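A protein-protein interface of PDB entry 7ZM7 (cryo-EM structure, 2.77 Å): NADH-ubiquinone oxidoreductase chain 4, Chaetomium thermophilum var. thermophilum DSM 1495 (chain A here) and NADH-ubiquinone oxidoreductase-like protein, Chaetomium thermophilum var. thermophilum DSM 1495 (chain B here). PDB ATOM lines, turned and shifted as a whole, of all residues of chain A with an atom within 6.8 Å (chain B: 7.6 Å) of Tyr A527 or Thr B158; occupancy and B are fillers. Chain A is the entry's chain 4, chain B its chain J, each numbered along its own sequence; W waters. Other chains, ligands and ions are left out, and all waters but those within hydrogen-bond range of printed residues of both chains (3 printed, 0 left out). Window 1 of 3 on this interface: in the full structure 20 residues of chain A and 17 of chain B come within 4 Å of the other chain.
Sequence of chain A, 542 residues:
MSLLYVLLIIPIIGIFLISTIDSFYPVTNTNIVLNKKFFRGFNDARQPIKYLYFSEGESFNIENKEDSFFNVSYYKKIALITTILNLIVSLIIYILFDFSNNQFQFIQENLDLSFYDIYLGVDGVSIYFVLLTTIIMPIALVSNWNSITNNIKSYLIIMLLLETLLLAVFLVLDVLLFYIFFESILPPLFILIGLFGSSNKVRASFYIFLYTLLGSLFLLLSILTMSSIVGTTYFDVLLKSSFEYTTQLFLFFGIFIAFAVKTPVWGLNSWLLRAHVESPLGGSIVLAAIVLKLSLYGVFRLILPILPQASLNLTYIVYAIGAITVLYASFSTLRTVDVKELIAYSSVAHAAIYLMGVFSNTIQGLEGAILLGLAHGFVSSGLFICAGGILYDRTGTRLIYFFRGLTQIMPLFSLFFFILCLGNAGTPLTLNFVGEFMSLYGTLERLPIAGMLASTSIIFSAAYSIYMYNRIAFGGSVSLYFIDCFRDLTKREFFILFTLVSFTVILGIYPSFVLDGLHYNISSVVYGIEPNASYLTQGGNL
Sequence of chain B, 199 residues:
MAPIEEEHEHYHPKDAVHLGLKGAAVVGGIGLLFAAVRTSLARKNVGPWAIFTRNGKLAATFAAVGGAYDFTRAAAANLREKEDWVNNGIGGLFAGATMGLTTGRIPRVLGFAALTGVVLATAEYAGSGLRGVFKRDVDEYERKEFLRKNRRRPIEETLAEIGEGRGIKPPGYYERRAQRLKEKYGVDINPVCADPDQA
Of the 16 printed residues of chain A, 7 touch a printed residue of chain B. Hydrophobic or aromatic side chains of chain A within 4 Å of the printed part of chain B: Tyr A245, Leu A312 and Tyr A527. Hydrophobic or aromatic side chains of chain B that line the printed part of chain A: Ile B162 and Ile B168. Along chain B the printed residues that touch a printed residue of chain A span positions 153 to 168.
Tyr A527 touches just these residues of chain B: Thr B158 (3.6 Å) and Ile B168 (3.9 Å). Of chain A, only Gln A309 and Tyr A527 come within 4 Å of Thr B158. Printed residues of chain B within 4 Å of Gln A309: Thr B158 (3.7 Å) and Ile B162 (3.7 Å). Of the printed residues of chain A, Glu B161 touches Tyr A245 (3.3 Å). Printed residues of chain B within 4 Å of Leu A312: Arg B166 (3.1 Å) and Ile B168 (3.9 Å). Printed residues of chain A within 4 Å of Ile B168: Leu A312 (3.9 Å), Tyr A527 (3.9 Å), Gly A528 (3.7 Å) and Ile A529 (3.9 Å). The nearest residue of chain B that does not touch Tyr A527 is Ile B162 (4.1 Å). The nearest residue of chain A that does not touch Thr B158 is Tyr A245 (6.6 Å).
Water W3 bridges the side-chain amide nitrogen of Gln A309 and the side-chain hydroxyl of Thr B158. Water W1 lies within hydrogen-bond range of OE1 of Gln A309, NH2 of Arg B153 and NE2 of Gln A248. Water W2 bridges the backbone carbonyl oxygen (O) of Leu A312 (2.9 Å) and the guanidinium group (NH2) of Arg B166 (3.4 Å).
The guanidinium group of Arg B153 lies within salt-bridge range of the side-chain carboxylate of Glu B157 (3.2 Å). The backbone carbonyl oxygen (O) of Ile B162 lies within hydrogen-bond range of the guanidinium group (NH1) of Arg B166 (3.1 Å). The side-chain amide oxygen (OE1) of Gln A248 lies within hydrogen-bond range of the backbone NH (N) of Gln A309, at 3.3 Å. The side-chain amide nitrogen (NE2) of Gln A309 sits at hydrogen-bond distance from the side-chain hydroxyl (OH) of Tyr A527. The backbone NH of Tyr A527 lies within hydrogen-bond range of the side-chain amide oxygen of Asn A361 (2.8 Å).
CD2 of Tyr A245 touches OE1 of Glu B161, 3.3 Å away. CG2 of Thr B158 touches CD of Gln A309 (3.7 Å). CB of Gln A309 touches CG2 of Ile B162, 3.7 Å away. Leu A312 touches Ile B168 (CD2 to CG1, 3.9 Å). OH of Tyr A527 touches CG2 of Thr B158, at 3.6 Å. CD1 of Ile B168 touches CD2 of Tyr A527 (3.9 Å). Gly A528 touches Gly B167. Ile B168 touches Gly A528 (CD1 to CA, 3.7 Å). O of Ile A529 touches C of Ile B168, 3.9 Å away.
The backbone carbonyl oxygen (O) of Ser A242 is in hydrogen-bond range of the guanidinium group (NH2) of Arg B153, at 2.7 Å. NH2 of Arg B166 is in hydrogen-bond range of O of Leu A312 (3.1 Å). The backbone carbonyl oxygen of Gly B167 is in hydrogen-bond range of the backbone NH of Ile A529 (3.4 Å).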
ATOM      1  N   SER A 242     -15.855 -14.638 -18.320  1.00  0.00           N
ATOM      2  CA  SER A 242     -15.132 -13.716 -17.418  1.00  0.00           C
ATOM      3  C   SER A 242     -16.052 -12.585 -16.941  1.00  0.00           C
ATOM      4  O   SER A 242     -16.436 -11.742 -17.761  1.00  0.00           O
ATOM      5  CB  SER A 242     -13.897 -13.196 -18.063  1.00  0.00           C
ATOM      6  OG  SER A 242     -13.229 -12.282 -17.206  1.00  0.00           O
ATOM      7  N   TYR A 245     -15.098  -6.666 -13.375  1.00  0.00           N
ATOM      8  CA  TYR A 245     -14.389  -6.484 -12.084  1.00  0.00           C
ATOM      9  C   TYR A 245     -15.360  -6.185 -10.943  1.00  0.00           C
ATOM     10  O   TYR A 245     -15.219  -6.797  -9.873  1.00  0.00           O
ATOM     11  CB  TYR A 245     -13.360  -5.359 -12.193  1.00  0.00           C
ATOM     12  CG  TYR A 245     -12.604  -5.082 -10.919  1.00  0.00           C
ATOM     13  CD1 TYR A 245     -11.586  -5.920 -10.496  1.00  0.00           C
ATOM     14  CD2 TYR A 245     -12.913  -3.987 -10.131  1.00  0.00           C
ATOM     15  CE1 TYR A 245     -10.889  -5.673  -9.324  1.00  0.00           C
ATOM     16  CE2 TYR A 245     -12.229  -3.727  -8.957  1.00  0.00           C
ATOM     17  CZ  TYR A 245     -11.213  -4.572  -8.552  1.00  0.00           C
ATOM     18  OH  TYR A 245     -10.538  -4.314  -7.395  1.00  0.00           O
ATOM     19  N   GLN A 248     -17.289  -9.154  -9.875  1.00  0.00           N
ATOM     20  CA  GLN A 248     -16.380 -10.144  -9.256  1.00  0.00           C
ATOM     21  C   GLN A 248     -16.029  -9.632  -7.875  1.00  0.00           C
ATOM     22  O   GLN A 248     -15.920 -10.459  -6.971  1.00  0.00           O
ATOM     23  CB  GLN A 248     -15.050 -10.117 -10.009  1.00  0.00           C
ATOM     24  CG  GLN A 248     -15.040 -10.817 -11.356  1.00  0.00           C
ATOM     25  CD  GLN A 248     -13.633 -10.948 -11.885  1.00  0.00           C
ATOM     26  OE1 GLN A 248     -12.663 -10.890 -11.138  1.00  0.00           O
ATOM     27  NE2 GLN A 248     -13.506 -11.136 -13.185  1.00  0.00           N
ATOM     28  N   LEU A 304     -10.842 -19.158  -7.612  1.00  0.00           N
ATOM     29  CA  LEU A 304      -9.619 -19.063  -8.402  1.00  0.00           C
ATOM     30  C   LEU A 304      -9.872 -18.921  -9.896  1.00  0.00           C
ATOM     31  O   LEU A 304      -9.260 -18.035 -10.512  1.00  0.00           O
ATOM     32  CB  LEU A 304      -8.718 -20.259  -8.094  1.00  0.00           C
ATOM     33  CG  LEU A 304      -8.253 -20.320  -6.654  1.00  0.00           C
ATOM     34  CD1 LEU A 304      -7.128 -21.319  -6.498  1.00  0.00           C
ATOM     35  CD2 LEU A 304      -7.856 -18.951  -6.182  1.00  0.00           C
ATOM     36  N   PRO A 305     -10.736 -19.725 -10.542  1.00  0.00           N
ATOM     37  CA  PRO A 305     -10.868 -19.608 -11.998  1.00  0.00           C
ATOM     38  C   PRO A 305     -11.853 -18.557 -12.503  1.00  0.00           C
ATOM     39  O   PRO A 305     -11.668 -18.054 -13.609  1.00  0.00           O
ATOM     40  CB  PRO A 305     -11.304 -21.017 -12.403  1.00  0.00           C
ATOM     41  CG  PRO A 305     -12.063 -21.488 -11.287  1.00  0.00           C
ATOM     42  CD  PRO A 305     -11.505 -20.874 -10.040  1.00  0.00           C
ATOM     43  N   PRO A 308     -10.730 -14.036 -10.742  1.00  0.00           N
ATOM     44  CA  PRO A 308      -9.300 -13.818 -10.525  1.00  0.00           C
ATOM     45  C   PRO A 308      -8.875 -12.396 -10.125  1.00  0.00           C
ATOM     46  O   PRO A 308      -8.015 -12.287  -9.279  1.00  0.00           O
ATOM     47  CB  PRO A 308      -8.708 -14.208 -11.878  1.00  0.00           C
ATOM     48  CG  PRO A 308      -9.735 -13.789 -12.872  1.00  0.00           C
ATOM     49  CD  PRO A 308     -11.001 -14.238 -12.192  1.00  0.00           C
ATOM     50  N   GLN A 309      -9.457 -11.363 -10.738  1.00  0.00           N
ATOM     51  CA  GLN A 309      -9.074  -9.961 -10.459  1.00  0.00           C
ATOM     52  C   GLN A 309      -9.454  -9.601  -9.026  1.00  0.00           C
ATOM     53  O   GLN A 309      -8.679  -8.890  -8.368  1.00  0.00           O
ATOM     54  CB  GLN A 309      -9.625  -9.053 -11.546  1.00  0.00           C
ATOM     55  CG  GLN A 309      -9.064  -9.381 -12.915  1.00  0.00           C
ATOM     56  CD  GLN A 309     -10.082  -9.132 -13.994  1.00  0.00           C
ATOM     57  OE1 GLN A 309     -10.861  -8.186 -13.928  1.00  0.00           O
ATOM     58  NE2 GLN A 309     -10.083  -9.994 -14.996  1.00  0.00           N
ATOM     59  N   LEU A 312      -7.064 -11.374  -6.583  1.00  0.00           N
ATOM     60  CA  LEU A 312      -5.770 -10.699  -6.590  1.00  0.00           C
ATOM     61  C   LEU A 312      -5.790  -9.406  -5.782  1.00  0.00           C
ATOM     62  O   LEU A 312      -4.899  -9.163  -4.967  1.00  0.00           O
ATOM     63  CB  LEU A 312      -5.355 -10.415  -8.032  1.00  0.00           C
ATOM     64  CG  LEU A 312      -3.920  -9.999  -8.321  1.00  0.00           C
ATOM     65  CD1 LEU A 312      -2.947 -11.042  -7.849  1.00  0.00           C
ATOM     66  CD2 LEU A 312      -3.761  -9.780  -9.788  1.00  0.00           C
ATOM     67  N   ASN A 361      -1.548 -17.369  -5.600  1.00  0.00           N
ATOM     68  CA  ASN A 361      -1.373 -17.267  -7.075  1.00  0.00           C
ATOM     69  C   ASN A 361      -0.067 -17.943  -7.463  1.00  0.00           C
ATOM     70  O   ASN A 361       0.533 -17.557  -8.467  1.00  0.00           O
ATOM     71  CB  ASN A 361      -1.544 -15.851  -7.627  1.00  0.00           C
ATOM     72  CG  ASN A 361      -2.417 -15.819  -8.859  1.00  0.00           C
ATOM     73  OD1 ASN A 361      -2.834 -16.862  -9.347  1.00  0.00           O
ATOM     74  ND2 ASN A 361      -2.697 -14.627  -9.355  1.00  0.00           N
ATOM     75  N   THR A 362       0.332 -18.939  -6.694  1.00  0.00           N
ATOM     76  CA  THR A 362       1.597 -19.655  -6.966  1.00  0.00           C
ATOM     77  C   THR A 362       1.257 -21.139  -7.079  1.00  0.00           C
ATOM     78  O   THR A 362       0.344 -21.576  -6.385  1.00  0.00           O
ATOM     79  CB  THR A 362       2.637 -19.342  -5.884  1.00  0.00           C
ATOM     80  OG1 THR A 362       2.766 -17.925  -5.764  1.00  0.00           O
ATOM     81  CG2 THR A 362       3.998 -19.934  -6.167  1.00  0.00           C
ATOM     82  N   SER A 524      -4.119 -24.921 -13.862  1.00  0.00           N
ATOM     83  CA  SER A 524      -5.149 -24.132 -14.513  1.00  0.00           C
ATOM     84  C   SER A 524      -5.925 -23.232 -13.561  1.00  0.00           C
ATOM     85  O   SER A 524      -6.943 -22.672 -13.972  1.00  0.00           O
ATOM     86  CB  SER A 524      -6.101 -25.054 -15.269  1.00  0.00           C
ATOM     87  OG  SER A 524      -6.674 -26.021 -14.422  1.00  0.00           O
ATOM     88  N   VAL A 525      -5.490 -23.062 -12.317  1.00  0.00           N
ATOM     89  CA  VAL A 525      -6.065 -22.030 -11.461  1.00  0.00           C
ATOM     90  C   VAL A 525      -5.104 -20.897 -11.195  1.00  0.00           C
ATOM     91  O   VAL A 525      -5.447 -19.998 -10.423  1.00  0.00           O
ATOM     92  CB  VAL A 525      -6.596 -22.590 -10.123  1.00  0.00           C
ATOM     93  CG1 VAL A 525      -7.813 -23.445 -10.342  1.00  0.00           C
ATOM     94  CG2 VAL A 525      -5.524 -23.369  -9.385  1.00  0.00           C
ATOM     95  N   VAL A 526      -3.926 -20.889 -11.801  1.00  0.00           N
ATOM     96  CA  VAL A 526      -3.007 -19.768 -11.611  1.00  0.00           C
ATOM     97  C   VAL A 526      -3.359 -18.642 -12.572  1.00  0.00           C
ATOM     98  O   VAL A 526      -3.668 -18.872 -13.741  1.00  0.00           O
ATOM     99  CB  VAL A 526      -1.540 -20.203 -11.780  1.00  0.00           C
ATOM    100  CG1 VAL A 526      -0.642 -19.051 -11.453  1.00  0.00           C
ATOM    101  CG2 VAL A 526      -1.206 -21.369 -10.889  1.00  0.00           C
ATOM    102  N   TYR A 527      -3.304 -17.414 -12.071  1.00  0.00           N
ATOM    103  CA  TYR A 527      -3.611 -16.209 -12.830  1.00  0.00           C
ATOM    104  C   TYR A 527      -2.335 -15.402 -13.010  1.00  0.00           C
ATOM    105  O   TYR A 527      -1.792 -14.886 -12.033  1.00  0.00           O
ATOM    106  CB  TYR A 527      -4.666 -15.390 -12.099  1.00  0.00           C
ATOM    107  CG  TYR A 527      -5.266 -14.240 -12.855  1.00  0.00           C
ATOM    108  CD1 TYR A 527      -5.980 -14.448 -14.011  1.00  0.00           C
ATOM    109  CD2 TYR A 527      -5.150 -12.943 -12.380  1.00  0.00           C
ATOM    110  CE1 TYR A 527      -6.544 -13.402 -14.683  1.00  0.00           C
ATOM    111  CE2 TYR A 527      -5.711 -11.898 -13.041  1.00  0.00           C
ATOM    112  CZ  TYR A 527      -6.406 -12.126 -14.200  1.00  0.00           C
ATOM    113  OH  TYR A 527      -6.976 -11.079 -14.880  1.00  0.00           O
ATOM    114  N   GLY A 528      -1.859 -15.289 -14.238  1.00  0.00           N
ATOM    115  CA  GLY A 528      -0.751 -14.397 -14.506  1.00  0.00           C
ATOM    116  C   GLY A 528      -0.078 -14.681 -15.827  1.00  0.00           C
ATOM    117  O   GLY A 528      -0.329 -15.676 -16.487  1.00  0.00           O
ATOM    118  N   ILE A 529       0.810 -13.764 -16.196  1.00  0.00           N
ATOM    119  CA  ILE A 529       1.642 -13.887 -17.384  1.00  0.00           C
ATOM    120  C   ILE A 529       3.023 -13.354 -17.062  1.00  0.00           C
ATOM    121  O   ILE A 529       3.191 -12.523 -16.170  1.00  0.00           O
ATOM    122  CB  ILE A 529       1.051 -13.145 -18.611  1.00  0.00           C
ATOM    123  CG1 ILE A 529       0.927 -11.653 -18.339  1.00  0.00           C
ATOM    124  CG2 ILE A 529      -0.235 -13.741 -19.072  1.00  0.00           C
ATOM    125  CD1 ILE A 529       0.586 -10.883 -19.549  1.00  0.00           C
ATOM    126  N   ARG B 152     -13.357 -12.384 -23.700  1.00  0.00           N
ATOM    127  CA  ARG B 152     -12.009 -11.780 -23.619  1.00  0.00           C
ATOM    128  C   ARG B 152     -12.130 -10.275 -23.557  1.00  0.00           C
ATOM    129  O   ARG B 152     -13.124  -9.745 -24.067  1.00  0.00           O
ATOM    130  CB  ARG B 152     -11.081 -12.150 -24.772  1.00  0.00           C
ATOM    131  CG  ARG B 152     -11.110 -13.598 -25.220  1.00  0.00           C
ATOM    132  CD  ARG B 152     -10.128 -13.700 -26.371  1.00  0.00           C
ATOM    133  NE  ARG B 152      -8.740 -13.595 -25.948  1.00  0.00           N
ATOM    134  CZ  ARG B 152      -7.699 -13.786 -26.750  1.00  0.00           C
ATOM    135  NH1 ARG B 152      -7.895 -14.074 -28.024  1.00  0.00           N
ATOM    136  NH2 ARG B 152      -6.468 -13.682 -26.283  1.00  0.00           N
ATOM    137  N   ARG B 153     -11.109  -9.665 -22.971  1.00  0.00           N
ATOM    138  CA  ARG B 153     -11.120  -8.204 -22.803  1.00  0.00           C
ATOM    139  C   ARG B 153      -9.805  -7.618 -23.327  1.00  0.00           C
ATOM    140  O   ARG B 153      -8.857  -8.379 -23.484  1.00  0.00           O
ATOM    141  CB  ARG B 153     -11.406  -7.823 -21.347  1.00  0.00           C
ATOM    142  CG  ARG B 153     -12.846  -8.059 -20.916  1.00  0.00           C
ATOM    143  CD  ARG B 153     -12.989  -7.844 -19.424  1.00  0.00           C
ATOM    144  NE  ARG B 153     -14.372  -7.695 -19.005  1.00  0.00           N
ATOM    145  CZ  ARG B 153     -15.121  -8.694 -18.562  1.00  0.00           C
ATOM    146  NH1 ARG B 153     -16.374  -8.479 -18.208  1.00  0.00           N
ATOM    147  NH2 ARG B 153     -14.613  -9.909 -18.489  1.00  0.00           N
ATOM    148  N   PRO B 154      -9.713  -6.298 -23.619  1.00  0.00           N
ATOM    149  CA  PRO B 154      -8.462  -5.695 -24.037  1.00  0.00           C
ATOM    150  C   PRO B 154      -7.519  -5.698 -22.826  1.00  0.00           C
ATOM    151  O   PRO B 154      -7.938  -5.385 -21.733  1.00  0.00           O
ATOM    152  CB  PRO B 154      -8.876  -4.259 -24.363  1.00  0.00           C
ATOM    153  CG  PRO B 154     -10.138  -4.015 -23.586  1.00  0.00           C
ATOM    154  CD  PRO B 154     -10.830  -5.358 -23.560  1.00  0.00           C
ATOM    155  N   ILE B 155      -6.261  -6.091 -23.061  1.00  0.00           N
ATOM    156  CA  ILE B 155      -5.314  -6.199 -21.960  1.00  0.00           C
ATOM    157  C   ILE B 155      -5.279  -4.910 -21.151  1.00  0.00           C
ATOM    158  O   ILE B 155      -5.130  -4.934 -19.927  1.00  0.00           O
ATOM    159  CB  ILE B 155      -3.925  -6.575 -22.510  1.00  0.00           C
ATOM    160  CG1 ILE B 155      -3.009  -6.996 -21.382  1.00  0.00           C
ATOM    161  CG2 ILE B 155      -3.314  -5.450 -23.332  1.00  0.00           C
ATOM    162  CD1 ILE B 155      -3.462  -8.209 -20.770  1.00  0.00           C
ATOM    163  N   GLU B 156      -5.385  -3.762 -21.813  1.00  0.00           N
ATOM    164  CA  GLU B 156      -5.295  -2.445 -21.117  1.00  0.00           C
ATOM    165  C   GLU B 156      -6.431  -2.306 -20.113  1.00  0.00           C
ATOM    166  O   GLU B 156      -6.202  -1.724 -19.050  1.00  0.00           O
ATOM    167  CB  GLU B 156      -5.439  -1.304 -22.127  1.00  0.00           C
ATOM    168  CG  GLU B 156      -4.394  -1.320 -23.230  1.00  0.00           C
ATOM    169  CD  GLU B 156      -4.691  -2.229 -24.413  1.00  0.00           C
ATOM    170  OE1 GLU B 156      -5.766  -2.863 -24.420  1.00  0.00           O
ATOM    171  OE2 GLU B 156      -3.842  -2.304 -25.323  1.00  0.00           O
ATOM    172  N   GLU B 157      -7.601  -2.836 -20.448  1.00  0.00           N
ATOM    173  CA  GLU B 157      -8.784  -2.702 -19.575  1.00  0.00           C
ATOM    174  C   GLU B 157      -8.532  -3.387 -18.231  1.00  0.00           C
ATOM    175  O   GLU B 157      -8.798  -2.756 -17.193  1.00  0.00           O
ATOM    176  CB  GLU B 157      -9.965  -3.366 -20.283  1.00  0.00           C
ATOM    177  CG  GLU B 157     -11.200  -3.491 -19.409  1.00  0.00           C
ATOM    178  CD  GLU B 157     -12.360  -4.229 -20.051  1.00  0.00           C
ATOM    179  OE1 GLU B 157     -12.416  -4.268 -21.296  1.00  0.00           O
ATOM    180  OE2 GLU B 157     -13.199  -4.769 -19.306  1.00  0.00           O
ATOM    181  N   THR B 158      -8.064  -4.634 -18.253  1.00  0.00           N
ATOM    182  CA  THR B 158      -7.830  -5.386 -16.995  1.00  0.00           C
ATOM    183  C   THR B 158      -6.718  -4.706 -16.205  1.00  0.00           C
ATOM    184  O   THR B 158      -6.880  -4.560 -14.982  1.00  0.00           O
ATOM    185  CB  THR B 158      -7.441  -6.837 -17.279  1.00  0.00           C
ATOM    186  OG1 THR B 158      -8.450  -7.388 -18.124  1.00  0.00           O
ATOM    187  CG2 THR B 158      -7.296  -7.673 -16.027  1.00  0.00           C
ATOM    188  N   LEU B 159      -5.684  -4.215 -16.883  1.00  0.00           N
ATOM    189  CA  LEU B 159      -4.519  -3.663 -16.150  1.00  0.00           C
ATOM    190  C   LEU B 159      -4.975  -2.504 -15.274  1.00  0.00           C
ATOM    191  O   LEU B 159      -4.385  -2.309 -14.220  1.00  0.00           O
ATOM    192  CB  LEU B 159      -3.433  -3.234 -17.135  1.00  0.00           C
ATOM    193  CG  LEU B 159      -2.677  -4.392 -17.783  1.00  0.00           C
ATOM    194  CD1 LEU B 159      -1.600  -3.889 -18.729  1.00  0.00           C
ATOM    195  CD2 LEU B 159      -2.087  -5.314 -16.729  1.00  0.00           C
ATOM    196  N   ALA B 160      -5.961  -1.729 -15.707  1.00  0.00           N
ATOM    197  CA  ALA B 160      -6.310  -0.559 -14.883  1.00  0.00           C
ATOM    198  C   ALA B 160      -6.775  -1.010 -13.495  1.00  0.00           C
ATOM    199  O   ALA B 160      -6.301  -0.424 -12.504  1.00  0.00           O
ATOM    200  CB  ALA B 160      -7.386   0.230 -15.579  1.00  0.00           C
ATOM    201  N   GLU B 161      -7.666  -2.005 -13.420  1.00  0.00           N
ATOM    202  CA  GLU B 161      -8.217  -2.420 -12.103  1.00  0.00           C
ATOM    203  C   GLU B 161      -7.157  -3.113 -11.246  1.00  0.00           C
ATOM    204  O   GLU B 161      -7.103  -2.809 -10.045  1.00  0.00           O
ATOM    205  CB  GLU B 161      -9.469  -3.283 -12.280  1.00  0.00           C
ATOM    206  CG  GLU B 161     -10.506  -2.686 -13.209  1.00  0.00           C
ATOM    207  CD  GLU B 161     -11.463  -1.706 -12.555  1.00  0.00           C
ATOM    208  OE1 GLU B 161     -11.285  -1.416 -11.356  1.00  0.00           O
ATOM    209  OE2 GLU B 161     -12.393  -1.242 -13.244  1.00  0.00           O
ATOM    210  N   ILE B 162      -6.366  -4.021 -11.830  1.00  0.00           N
ATOM    211  CA  ILE B 162      -5.398  -4.796 -11.004  1.00  0.00           C
ATOM    212  C   ILE B 162      -4.012  -4.154 -11.029  1.00  0.00           C
ATOM    213  O   ILE B 162      -3.360  -4.142  -9.971  1.00  0.00           O
ATOM    214  CB  ILE B 162      -5.369  -6.285 -11.394  1.00  0.00           C
ATOM    215  CG1 ILE B 162      -5.092  -6.506 -12.883  1.00  0.00           C
ATOM    216  CG2 ILE B 162      -6.650  -6.969 -10.947  1.00  0.00           C
ATOM    217  CD1 ILE B 162      -4.722  -7.928 -13.224  1.00  0.00           C
ATOM    218  N   GLY B 163      -3.569  -3.671 -12.183  1.00  0.00           N
ATOM    219  CA  GLY B 163      -2.216  -3.100 -12.312  1.00  0.00           C
ATOM    220  C   GLY B 163      -1.191  -4.131 -12.742  1.00  0.00           C
ATOM    221  O   GLY B 163      -1.339  -5.302 -12.351  1.00  0.00           O
ATOM    222  N   GLU B 164      -0.176  -3.717 -13.498  1.00  0.00           N
ATOM    223  CA  GLU B 164       0.937  -4.625 -13.872  1.00  0.00           C
ATOM    224  C   GLU B 164       1.760  -4.899 -12.617  1.00  0.00           C
ATOM    225  O   GLU B 164       1.955  -3.955 -11.832  1.00  0.00           O
ATOM    226  CB  GLU B 164       1.861  -3.994 -14.913  1.00  0.00           C
ATOM    227  CG  GLU B 164       1.136  -3.354 -16.084  1.00  0.00           C
ATOM    228  CD  GLU B 164       0.723  -1.902 -15.905  1.00  0.00           C
ATOM    229  OE1 GLU B 164       0.025  -1.377 -16.794  1.00  0.00           O
ATOM    230  OE2 GLU B 164       1.101  -1.297 -14.880  1.00  0.00           O
ATOM    231  N   ARG B 166       2.727  -8.004  -9.331  1.00  0.00           N
ATOM    232  CA  ARG B 166       2.084  -9.094  -8.549  1.00  0.00           C
ATOM    233  C   ARG B 166       1.885 -10.301  -9.466  1.00  0.00           C
ATOM    234  O   ARG B 166       0.784 -10.872  -9.448  1.00  0.00           O
ATOM    235  CB  ARG B 166       0.853  -8.618  -7.773  1.00  0.00           C
ATOM    236  CG  ARG B 166       1.170  -7.577  -6.711  1.00  0.00           C
ATOM    237  CD  ARG B 166      -0.069  -7.090  -5.994  1.00  0.00           C
ATOM    238  NE  ARG B 166      -1.056  -6.646  -6.960  1.00  0.00           N
ATOM    239  CZ  ARG B 166      -2.353  -6.554  -6.717  1.00  0.00           C
ATOM    240  NH1 ARG B 166      -3.175  -6.144  -7.664  1.00  0.00           N
ATOM    241  NH2 ARG B 166      -2.824  -6.891  -5.534  1.00  0.00           N
ATOM    242  N   GLY B 167       2.897 -10.627 -10.277  1.00  0.00           N
ATOM    243  CA  GLY B 167       2.844 -11.820 -11.143  1.00  0.00           C
ATOM    244  C   GLY B 167       2.131 -11.544 -12.441  1.00  0.00           C
ATOM    245  O   GLY B 167       2.013 -12.469 -13.252  1.00  0.00           O
ATOM    246  N   ILE B 168       1.603 -10.336 -12.593  1.00  0.00           N
ATOM    247  CA  ILE B 168       1.028  -9.958 -13.903  1.00  0.00           C
ATOM    248  C   ILE B 168       2.127  -9.146 -14.573  1.00  0.00           C
ATOM    249  O   ILE B 168       2.180  -7.939 -14.343  1.00  0.00           O
ATOM    250  CB  ILE B 168      -0.273  -9.157 -13.729  1.00  0.00           C
ATOM    251  CG1 ILE B 168      -1.231  -9.831 -12.745  1.00  0.00           C
ATOM    252  CG2 ILE B 168      -0.932  -8.893 -15.075  1.00  0.00           C
ATOM    253  CD1 ILE B 168      -1.856 -11.099 -13.268  1.00  0.00           C
HETATM  254  O   HOH W   1     -13.057  -8.817 -15.675  1.00  0.00           O
HETATM  255  O   HOH W   2      -3.837  -8.072  -2.519  1.00  0.00           O
HETATM  256  O   HOH W   3     -10.726  -9.229 -17.647  1.00  0.00           O
